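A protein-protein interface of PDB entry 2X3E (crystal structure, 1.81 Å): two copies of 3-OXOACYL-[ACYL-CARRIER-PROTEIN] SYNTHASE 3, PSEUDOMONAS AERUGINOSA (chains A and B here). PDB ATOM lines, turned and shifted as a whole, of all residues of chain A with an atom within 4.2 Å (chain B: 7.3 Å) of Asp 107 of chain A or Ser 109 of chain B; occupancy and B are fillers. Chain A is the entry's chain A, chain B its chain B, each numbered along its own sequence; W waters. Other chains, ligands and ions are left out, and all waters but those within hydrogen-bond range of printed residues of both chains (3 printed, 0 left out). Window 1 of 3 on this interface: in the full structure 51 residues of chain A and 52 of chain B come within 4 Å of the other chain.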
ATOM      1  N   LEU A  78      -3.467  26.682  26.851  1.00  0.00           N
ATOM      2  CA  LEU A  78      -3.153  25.335  27.306  1.00  0.00           C
ATOM      3  C   LEU A  78      -4.022  24.334  26.571  1.00  0.00           C
ATOM      4  O   LEU A  78      -5.260  24.446  26.575  1.00  0.00           O
ATOM      5  CB  LEU A  78      -3.377  25.156  28.811  1.00  0.00           C
ATOM      6  CG  LEU A  78      -2.719  26.061  29.859  1.00  0.00           C
ATOM      7  CD1 LEU A  78      -2.535  25.287  31.170  1.00  0.00           C
ATOM      8  CD2 LEU A  78      -1.410  26.718  29.407  1.00  0.00           C
ATOM      9  N   THR A  80      -5.160  20.848  27.088  1.00  0.00           N
ATOM     10  CA  THR A  80      -5.255  19.924  28.229  1.00  0.00           C
ATOM     11  C   THR A  80      -6.644  19.302  28.366  1.00  0.00           C
ATOM     12  O   THR A  80      -7.645  19.902  27.967  1.00  0.00           O
ATOM     13  CB  THR A  80      -4.891  20.618  29.583  1.00  0.00           C
ATOM     14  OG1 THR A  80      -4.749  19.635  30.614  1.00  0.00           O
ATOM     15  CG2 THR A  80      -5.950  21.638  30.017  1.00  0.00           C
ATOM     16  N   ALA A  89     -10.896  27.927  33.239  1.00  0.00           N
ATOM     17  CA  ALA A  89      -9.736  27.349  32.585  1.00  0.00           C
ATOM     18  C   ALA A  89      -8.481  27.524  33.454  1.00  0.00           C
ATOM     19  O   ALA A  89      -8.445  28.340  34.383  1.00  0.00           O
ATOM     20  CB  ALA A  89      -9.535  27.998  31.212  1.00  0.00           C
ATOM     21  N   THR A  90      -7.454  26.741  33.151  1.00  0.00           N
ATOM     22  CA  THR A  90      -6.173  26.815  33.855  1.00  0.00           C
ATOM     23  C   THR A  90      -5.256  27.893  33.268  1.00  0.00           C
ATOM     24  O   THR A  90      -4.433  28.468  33.981  1.00  0.00           O
ATOM     25  CB  THR A  90      -5.483  25.436  33.822  1.00  0.00           C
ATOM     26  OG1 THR A  90      -6.337  24.483  34.464  1.00  0.00           O
ATOM     27  CG2 THR A  90      -4.125  25.464  34.540  1.00  0.00           C
ATOM     28  N   ALA A  91      -5.426  28.178  31.976  1.00  0.00           N
ATOM     29  CA  ALA A  91      -4.548  29.099  31.247  1.00  0.00           C
ATOM     30  C   ALA A  91      -4.446  30.496  31.866  1.00  0.00           C
ATOM     31  O   ALA A  91      -3.343  31.034  31.978  1.00  0.00           O
ATOM     32  CB  ALA A  91      -4.972  29.190  29.783  1.00  0.00           C
ATOM     33  N   PHE A 106      -6.822  30.839  27.362  1.00  0.00           N
ATOM     34  CA  PHE A 106      -7.873  29.820  27.409  1.00  0.00           C
ATOM     35  C   PHE A 106      -7.310  28.408  27.283  1.00  0.00           C
ATOM     36  O   PHE A 106      -6.169  28.235  26.860  1.00  0.00           O
ATOM     37  CB  PHE A 106      -8.934  30.083  26.315  1.00  0.00           C
ATOM     38  CG  PHE A 106      -8.429  29.930  24.887  1.00  0.00           C
ATOM     39  CD1 PHE A 106      -8.491  28.698  24.236  1.00  0.00           C
ATOM     40  CD2 PHE A 106      -7.941  31.029  24.180  1.00  0.00           C
ATOM     41  CE1 PHE A 106      -8.053  28.555  22.920  1.00  0.00           C
ATOM     42  CE2 PHE A 106      -7.509  30.905  22.866  1.00  0.00           C
ATOM     43  CZ  PHE A 106      -7.556  29.662  22.230  1.00  0.00           C
ATOM     44  N   ASP A 107      -8.115  27.413  27.668  1.00  0.00           N
ATOM     45  CA  ASP A 107      -7.762  25.992  27.522  1.00  0.00           C
ATOM     46  C   ASP A 107      -8.470  25.400  26.300  1.00  0.00           C
ATOM     47  O   ASP A 107      -9.621  25.753  26.013  1.00  0.00           O
ATOM     48  CB  ASP A 107      -8.163  25.174  28.761  1.00  0.00           C
ATOM     49  CG  ASP A 107      -7.407  25.567  30.029  1.00  0.00           C
ATOM     50  OD1 ASP A 107      -6.567  26.497  30.006  1.00  0.00           O
ATOM     51  OD2 ASP A 107      -7.672  24.934  31.087  1.00  0.00           O
ATOM     52  N   LEU A 108      -7.783  24.490  25.601  1.00  0.00           N
ATOM     53  CA  LEU A 108      -8.314  23.808  24.421  1.00  0.00           C
ATOM     54  C   LEU A 108      -8.368  22.317  24.716  1.00  0.00           C
ATOM     55  O   LEU A 108      -7.399  21.753  25.218  1.00  0.00           O
ATOM     56  CB  LEU A 108      -7.427  24.088  23.203  1.00  0.00           C
ATOM     57  CG  LEU A 108      -7.890  23.536  21.846  1.00  0.00           C
ATOM     58  CD1 LEU A 108      -7.411  24.447  20.712  1.00  0.00           C
ATOM     59  CD2 LEU A 108      -7.423  22.088  21.613  1.00  0.00           C
ATOM     60  N   LEU B  78     -17.248  24.141  20.636  1.00  0.00           N
ATOM     61  CA  LEU B  78     -18.104  24.409  21.787  1.00  0.00           C
ATOM     62  C   LEU B  78     -17.328  25.203  22.825  1.00  0.00           C
ATOM     63  O   LEU B  78     -16.309  24.731  23.351  1.00  0.00           O
ATOM     64  CB  LEU B  78     -18.639  23.132  22.439  1.00  0.00           C
ATOM     65  CG  LEU B  78     -19.463  22.091  21.678  1.00  0.00           C
ATOM     66  CD1 LEU B  78     -20.372  21.323  22.657  1.00  0.00           C
ATOM     67  CD2 LEU B  78     -20.257  22.652  20.536  1.00  0.00           C
ATOM     68  N   ALA B  79     -17.814  26.411  23.115  1.00  0.00           N
ATOM     69  CA  ALA B  79     -17.363  27.175  24.269  1.00  0.00           C
ATOM     70  C   ALA B  79     -18.182  26.717  25.468  1.00  0.00           C
ATOM     71  O   ALA B  79     -19.377  26.968  25.533  1.00  0.00           O
ATOM     72  CB  ALA B  79     -17.542  28.658  24.031  1.00  0.00           C
ATOM     73  N   THR B  80     -17.539  26.017  26.401  1.00  0.00           N
ATOM     74  CA  THR B  80     -18.243  25.422  27.531  1.00  0.00           C
ATOM     75  C   THR B  80     -17.290  25.161  28.685  1.00  0.00           C
ATOM     76  O   THR B  80     -16.085  24.977  28.472  1.00  0.00           O
ATOM     77  CB  THR B  80     -18.927  24.085  27.132  1.00  0.00           C
ATOM     78  OG1 THR B  80     -19.791  23.642  28.189  1.00  0.00           O
ATOM     79  CG2 THR B  80     -17.896  23.000  26.837  1.00  0.00           C
ATOM     80  N   SER B  81     -17.837  25.160  29.899  1.00  0.00           N
ATOM     81  CA  SER B  81     -17.119  24.738  31.109  1.00  0.00           C
ATOM     82  C   SER B  81     -17.802  23.521  31.725  1.00  0.00           C
ATOM     83  O   SER B  81     -17.459  23.113  32.837  1.00  0.00           O
ATOM     84  CB  SER B  81     -17.115  25.853  32.156  1.00  0.00           C
ATOM     85  OG  SER B  81     -16.629  27.065  31.624  1.00  0.00           O
ATOM     86  N   THR B  82     -18.776  22.960  31.004  1.00  0.00           N
ATOM     87  CA  THR B  82     -19.588  21.854  31.504  1.00  0.00           C
ATOM     88  C   THR B  82     -19.778  20.821  30.399  1.00  0.00           C
ATOM     89  O   THR B  82     -20.902  20.409  30.093  1.00  0.00           O
ATOM     90  CB  THR B  82     -20.961  22.343  32.004  1.00  0.00           C
ATOM     91  OG1 THR B  82     -21.559  23.177  31.004  1.00  0.00           O
ATOM     92  CG2 THR B  82     -20.818  23.113  33.307  1.00  0.00           C
ATOM     93  N   PHE B 106     -13.289  21.001  18.600  1.00  0.00           N
ATOM     94  CA  PHE B 106     -12.752  21.020  19.960  1.00  0.00           C
ATOM     95  C   PHE B 106     -13.619  21.878  20.892  1.00  0.00           C
ATOM     96  O   PHE B 106     -14.487  22.629  20.436  1.00  0.00           O
ATOM     97  CB  PHE B 106     -11.297  21.515  19.961  1.00  0.00           C
ATOM     98  CG  PHE B 106     -11.118  22.937  19.457  1.00  0.00           C
ATOM     99  CD1 PHE B 106     -11.160  24.008  20.339  1.00  0.00           C
ATOM    100  CD2 PHE B 106     -10.859  23.192  18.113  1.00  0.00           C
ATOM    101  CE1 PHE B 106     -10.978  25.318  19.897  1.00  0.00           C
ATOM    102  CE2 PHE B 106     -10.671  24.502  17.657  1.00  0.00           C
ATOM    103  CZ  PHE B 106     -10.731  25.562  18.550  1.00  0.00           C
ATOM    104  N   ASP B 107     -13.380  21.751  22.195  1.00  0.00           N
ATOM    105  CA  ASP B 107     -14.032  22.600  23.192  1.00  0.00           C
ATOM    106  C   ASP B 107     -13.051  23.673  23.665  1.00  0.00           C
ATOM    107  O   ASP B 107     -11.850  23.424  23.782  1.00  0.00           O
ATOM    108  CB  ASP B 107     -14.525  21.787  24.396  1.00  0.00           C
ATOM    109  CG  ASP B 107     -15.571  20.745  24.025  1.00  0.00           C
ATOM    110  OD1 ASP B 107     -15.974  20.668  22.840  1.00  0.00           O
ATOM    111  OD2 ASP B 107     -15.983  19.977  24.923  1.00  0.00           O
ATOM    112  N   LEU B 108     -13.583  24.865  23.922  1.00  0.00           N
ATOM    113  CA  LEU B 108     -12.802  26.001  24.394  1.00  0.00           C
ATOM    114  C   LEU B 108     -13.306  26.393  25.778  1.00  0.00           C
ATOM    115  O   LEU B 108     -14.511  26.511  25.989  1.00  0.00           O
ATOM    116  CB  LEU B 108     -12.933  27.173  23.415  1.00  0.00           C
ATOM    117  CG  LEU B 108     -12.125  28.435  23.729  1.00  0.00           C
ATOM    118  CD1 LEU B 108     -11.718  29.176  22.449  1.00  0.00           C
ATOM    119  CD2 LEU B 108     -12.892  29.366  24.670  1.00  0.00           C
ATOM    120  N   SER B 109     -12.380  26.589  26.717  1.00  0.00           N
ATOM    121  CA  SER B 109     -12.720  26.951  28.092  1.00  0.00           C
ATOM    122  C   SER B 109     -12.330  28.390  28.411  1.00  0.00           C
ATOM    123  O   SER B 109     -11.149  28.728  28.473  1.00  0.00           O
ATOM    124  CB  SER B 109     -12.051  25.992  29.085  1.00  0.00           C
ATOM    125  OG  SER B 109     -12.395  26.307  30.431  1.00  0.00           O
ATOM    126  N   ALA B 110     -13.340  29.236  28.587  1.00  0.00           N
ATOM    127  CA  ALA B 110     -13.141  30.590  29.102  1.00  0.00           C
ATOM    128  C   ALA B 110     -14.374  31.087  29.860  1.00  0.00           C
ATOM    129  O   ALA B 110     -14.670  32.285  29.863  1.00  0.00           O
ATOM    130  CB  ALA B 110     -12.775  31.545  27.970  1.00  0.00           C
ATOM    131  N   ALA B 111     -15.071  30.157  30.517  1.00  0.00           N
ATOM    132  CA  ALA B 111     -16.183  30.476  31.403  1.00  0.00           C
ATOM    133  C   ALA B 111     -17.210  31.391  30.727  1.00  0.00           C
ATOM    134  O   ALA B 111     -17.611  31.128  29.586  1.00  0.00           O
ATOM    135  CB  ALA B 111     -15.659  31.074  32.707  1.00  0.00           C
ATOM    136  N   THR B 113     -16.835  34.235  29.523  1.00  0.00           N
ATOM    137  CA  THR B 113     -16.264  34.900  28.346  1.00  0.00           C
ATOM    138  C   THR B 113     -16.090  33.941  27.160  1.00  0.00           C
ATOM    139  O   THR B 113     -15.549  34.326  26.132  1.00  0.00           O
ATOM    140  CB  THR B 113     -14.899  35.548  28.685  1.00  0.00           C
ATOM    141  OG1 THR B 113     -14.976  36.173  29.971  1.00  0.00           O
ATOM    142  CG2 THR B 113     -14.519  36.622  27.647  1.00  0.00           C
ATOM    143  N   GLY B 114     -16.556  32.703  27.300  1.00  0.00           N
ATOM    144  CA  GLY B 114     -16.332  31.657  26.304  1.00  0.00           C
ATOM    145  C   GLY B 114     -16.810  31.924  24.884  1.00  0.00           C
ATOM    146  O   GLY B 114     -16.157  31.518  23.932  1.00  0.00           O
ATOM    147  N   TYR B 117     -14.319  34.572  23.371  1.00  0.00           N
ATOM    148  CA  TYR B 117     -13.096  33.829  23.041  1.00  0.00           C
ATOM    149  C   TYR B 117     -13.325  32.875  21.869  1.00  0.00           C
ATOM    150  O   TYR B 117     -12.452  32.717  21.007  1.00  0.00           O
ATOM    151  CB  TYR B 117     -12.550  33.054  24.252  1.00  0.00           C
ATOM    152  CG  TYR B 117     -11.552  33.838  25.082  1.00  0.00           C
ATOM    153  CD1 TYR B 117     -11.971  34.728  26.064  1.00  0.00           C
ATOM    154  CD2 TYR B 117     -10.180  33.689  24.880  1.00  0.00           C
ATOM    155  CE1 TYR B 117     -11.055  35.454  26.828  1.00  0.00           C
ATOM    156  CE2 TYR B 117      -9.255  34.401  25.649  1.00  0.00           C
ATOM    157  CZ  TYR B 117      -9.703  35.286  26.619  1.00  0.00           C
ATOM    158  OH  TYR B 117      -8.789  35.994  27.370  1.00  0.00           O
ATOM    159  N   ALA B 312     -15.103  33.859  34.903  1.00  0.00           N
ATOM    160  CA  ALA B 312     -14.118  33.121  35.671  1.00  0.00           C
ATOM    161  C   ALA B 312     -12.803  33.022  34.904  1.00  0.00           C
ATOM    162  O   ALA B 312     -12.784  32.948  33.665  1.00  0.00           O
ATOM    163  CB  ALA B 312     -14.650  31.740  36.023  1.00  0.00           C
ATOM    164  N   THR B 315     -11.436  36.227  33.147  1.00  0.00           N
ATOM    165  CA  THR B 315     -11.347  36.470  31.711  1.00  0.00           C
ATOM    166  C   THR B 315     -12.245  37.634  31.322  1.00  0.00           C
ATOM    167  O   THR B 315     -13.195  37.959  32.027  1.00  0.00           O
ATOM    168  CB  THR B 315     -11.788  35.232  30.907  1.00  0.00           C
ATOM    169  OG1 THR B 315     -13.043  34.748  31.409  1.00  0.00           O
ATOM    170  CG2 THR B 315     -10.749  34.133  30.996  1.00  0.00           C
HETATM  171  O   HOH W   1     -13.894  27.885  31.961  1.00  0.00           O
HETATM  172  O   HOH W   2     -11.311  23.432  26.824  1.00  0.00           O
HETATM  173  O   HOH W   3     -11.373  30.791  32.241  1.00  0.00           O
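The backbone NH (N) of Leu 78 of chain A sits at hydrogen-bond distance from the backbone carbonyl oxygen (O) of Phe 106 of chain A, 3.1 Å away.
O of Leu 78 of chain A sits at hydrogen-bond distance from N of Leu 108 of chain A.
N of Thr 80 of chain A lies within hydrogen-bond range of O of Leu 108 of chain A.
The side-chain carboxylate (OD1) of Asp 107 of chain A lies within hydrogen-bond range of the backbone NH (N) of Ala 91 of chain A.
O of Phe 106 of chain B lies within hydrogen-bond range of N of Leu 78 of chain B (3.2 Å).
The backbone NH (N) of Leu 108 of chain B is in hydrogen-bond range of the backbone carbonyl oxygen (O) of Leu 78 of chain B, 2.8 Å away.
Printed residues of chain B that touch a printed residue of chain A: Phe 106, Asp 107, Leu 108, Ser 109 and Tyr 117.
Hydrophobic or aromatic side chains of chain B that line the printed part of chain A: Phe 106, Leu 108 and Tyr 117.
Among the printed residues, 9 pairs touch across the chains.
Among the printed residues, no Asp or Glu carboxylate lies within 4 Å of a Lys or Arg side-chain nitrogen of the other chain.
Phe 106 of chain A touches Leu 108 of chain B, and with the chains exchanged Leu 108 of chain A touches Phe 106 of chain B.
Asp 107 of chain A touches its own counterpart, Asp 107 of chain B.
Asp 107 of chain A touches Leu 108 of chain B, and with the chains exchanged Leu 108 of chain A touches Asp 107 of chain B.
Positions printed for both chains: 78, 80, 106, 107 and 108.
Of the 9 pairs that touch across the chains among the printed residues, 5 have their exchanged pair printed and touching as well.
The backbone carbonyl oxygen of Asp 107 of chain A lies within hydrogen-bond range of the backbone NH of Ser 109 of chain B (3.0 Å).
Water W1 lies within hydrogen-bond range of OG of Ser 109 of chain B, OG of Ser 81 of chain B, N of Ala 111 of chain B and N of Ala 89 of chain A.
Water W3 lies within hydrogen-bond range of O of Ala 312 of chain B (2.9 Å) and N of Ala 89 of chain A (3.1 Å).
Water W2 lies within hydrogen-bond range of the backbone carbonyl oxygen (O) of Asp 107 of chain A (3.0 Å), the backbone carbonyl oxygen (O) of Asp 107 of chain B (3.1 Å) and the backbone NH (N) of Ser 109 of chain B (3.3 Å).
CB of Ala 89 of chain A touches O of Ser 109 of chain B, at 3.3 Å.
Phe 106 of chain A touches Leu 108 of chain B.
CB of Phe 106 of chain A touches O of Ser 109 of chain B, at 3.4 Å.
CD2 of Tyr 117 of chain B touches CD2 of Phe 106 of chain A, at 3.5 Å.
O of Asp 107 of chain B touches O of Asp 107 of chain A, 3.9 Å away.
Asp 107 of chain A touches Leu 108 of chain B (O to CA, 3.6 Å).
Phe 106 of chain B touches Leu 108 of chain A.
Leu 108 of chain A touches Asp 107 of chain B.
Of the printed residues of chain B, Ala 89 of chain A touches Ser 109 (3.3 Å).
Of the printed residues of chain B, Asp 107 of chain A touches Asp 107 (3.9 Å), Leu 108 (3.6 Å) and Ser 109 (3.0 Å).
Printed residues of chain B within 4 Å of Leu 108 of chain A: Phe 106 (3.6 Å) and Asp 107 (3.6 Å).
Printed residues of chain A within 4 Å of Phe 106 of chain B: Leu 108.
Of the printed residues of chain A, Asp 107 of chain B touches Asp 107 (3.9 Å) and Leu 108 (3.6 Å).
Of the printed residues of chain A, Leu 108 of chain B touches Phe 106 and Asp 107.
Ser 109 of chain B touches just these residues of chain A: Ala 89 (3.3 Å), Phe 106 (3.4 Å) and Asp 107 (3.0 Å).
The nearest residue of chain B that does not touch Asp 107 of chain A is Ala 110 of chain B (5.6 Å).
The nearest printed residue of chain B that does not touch Leu 108 of chain A is Leu 108 of chain B (5.0 Å).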
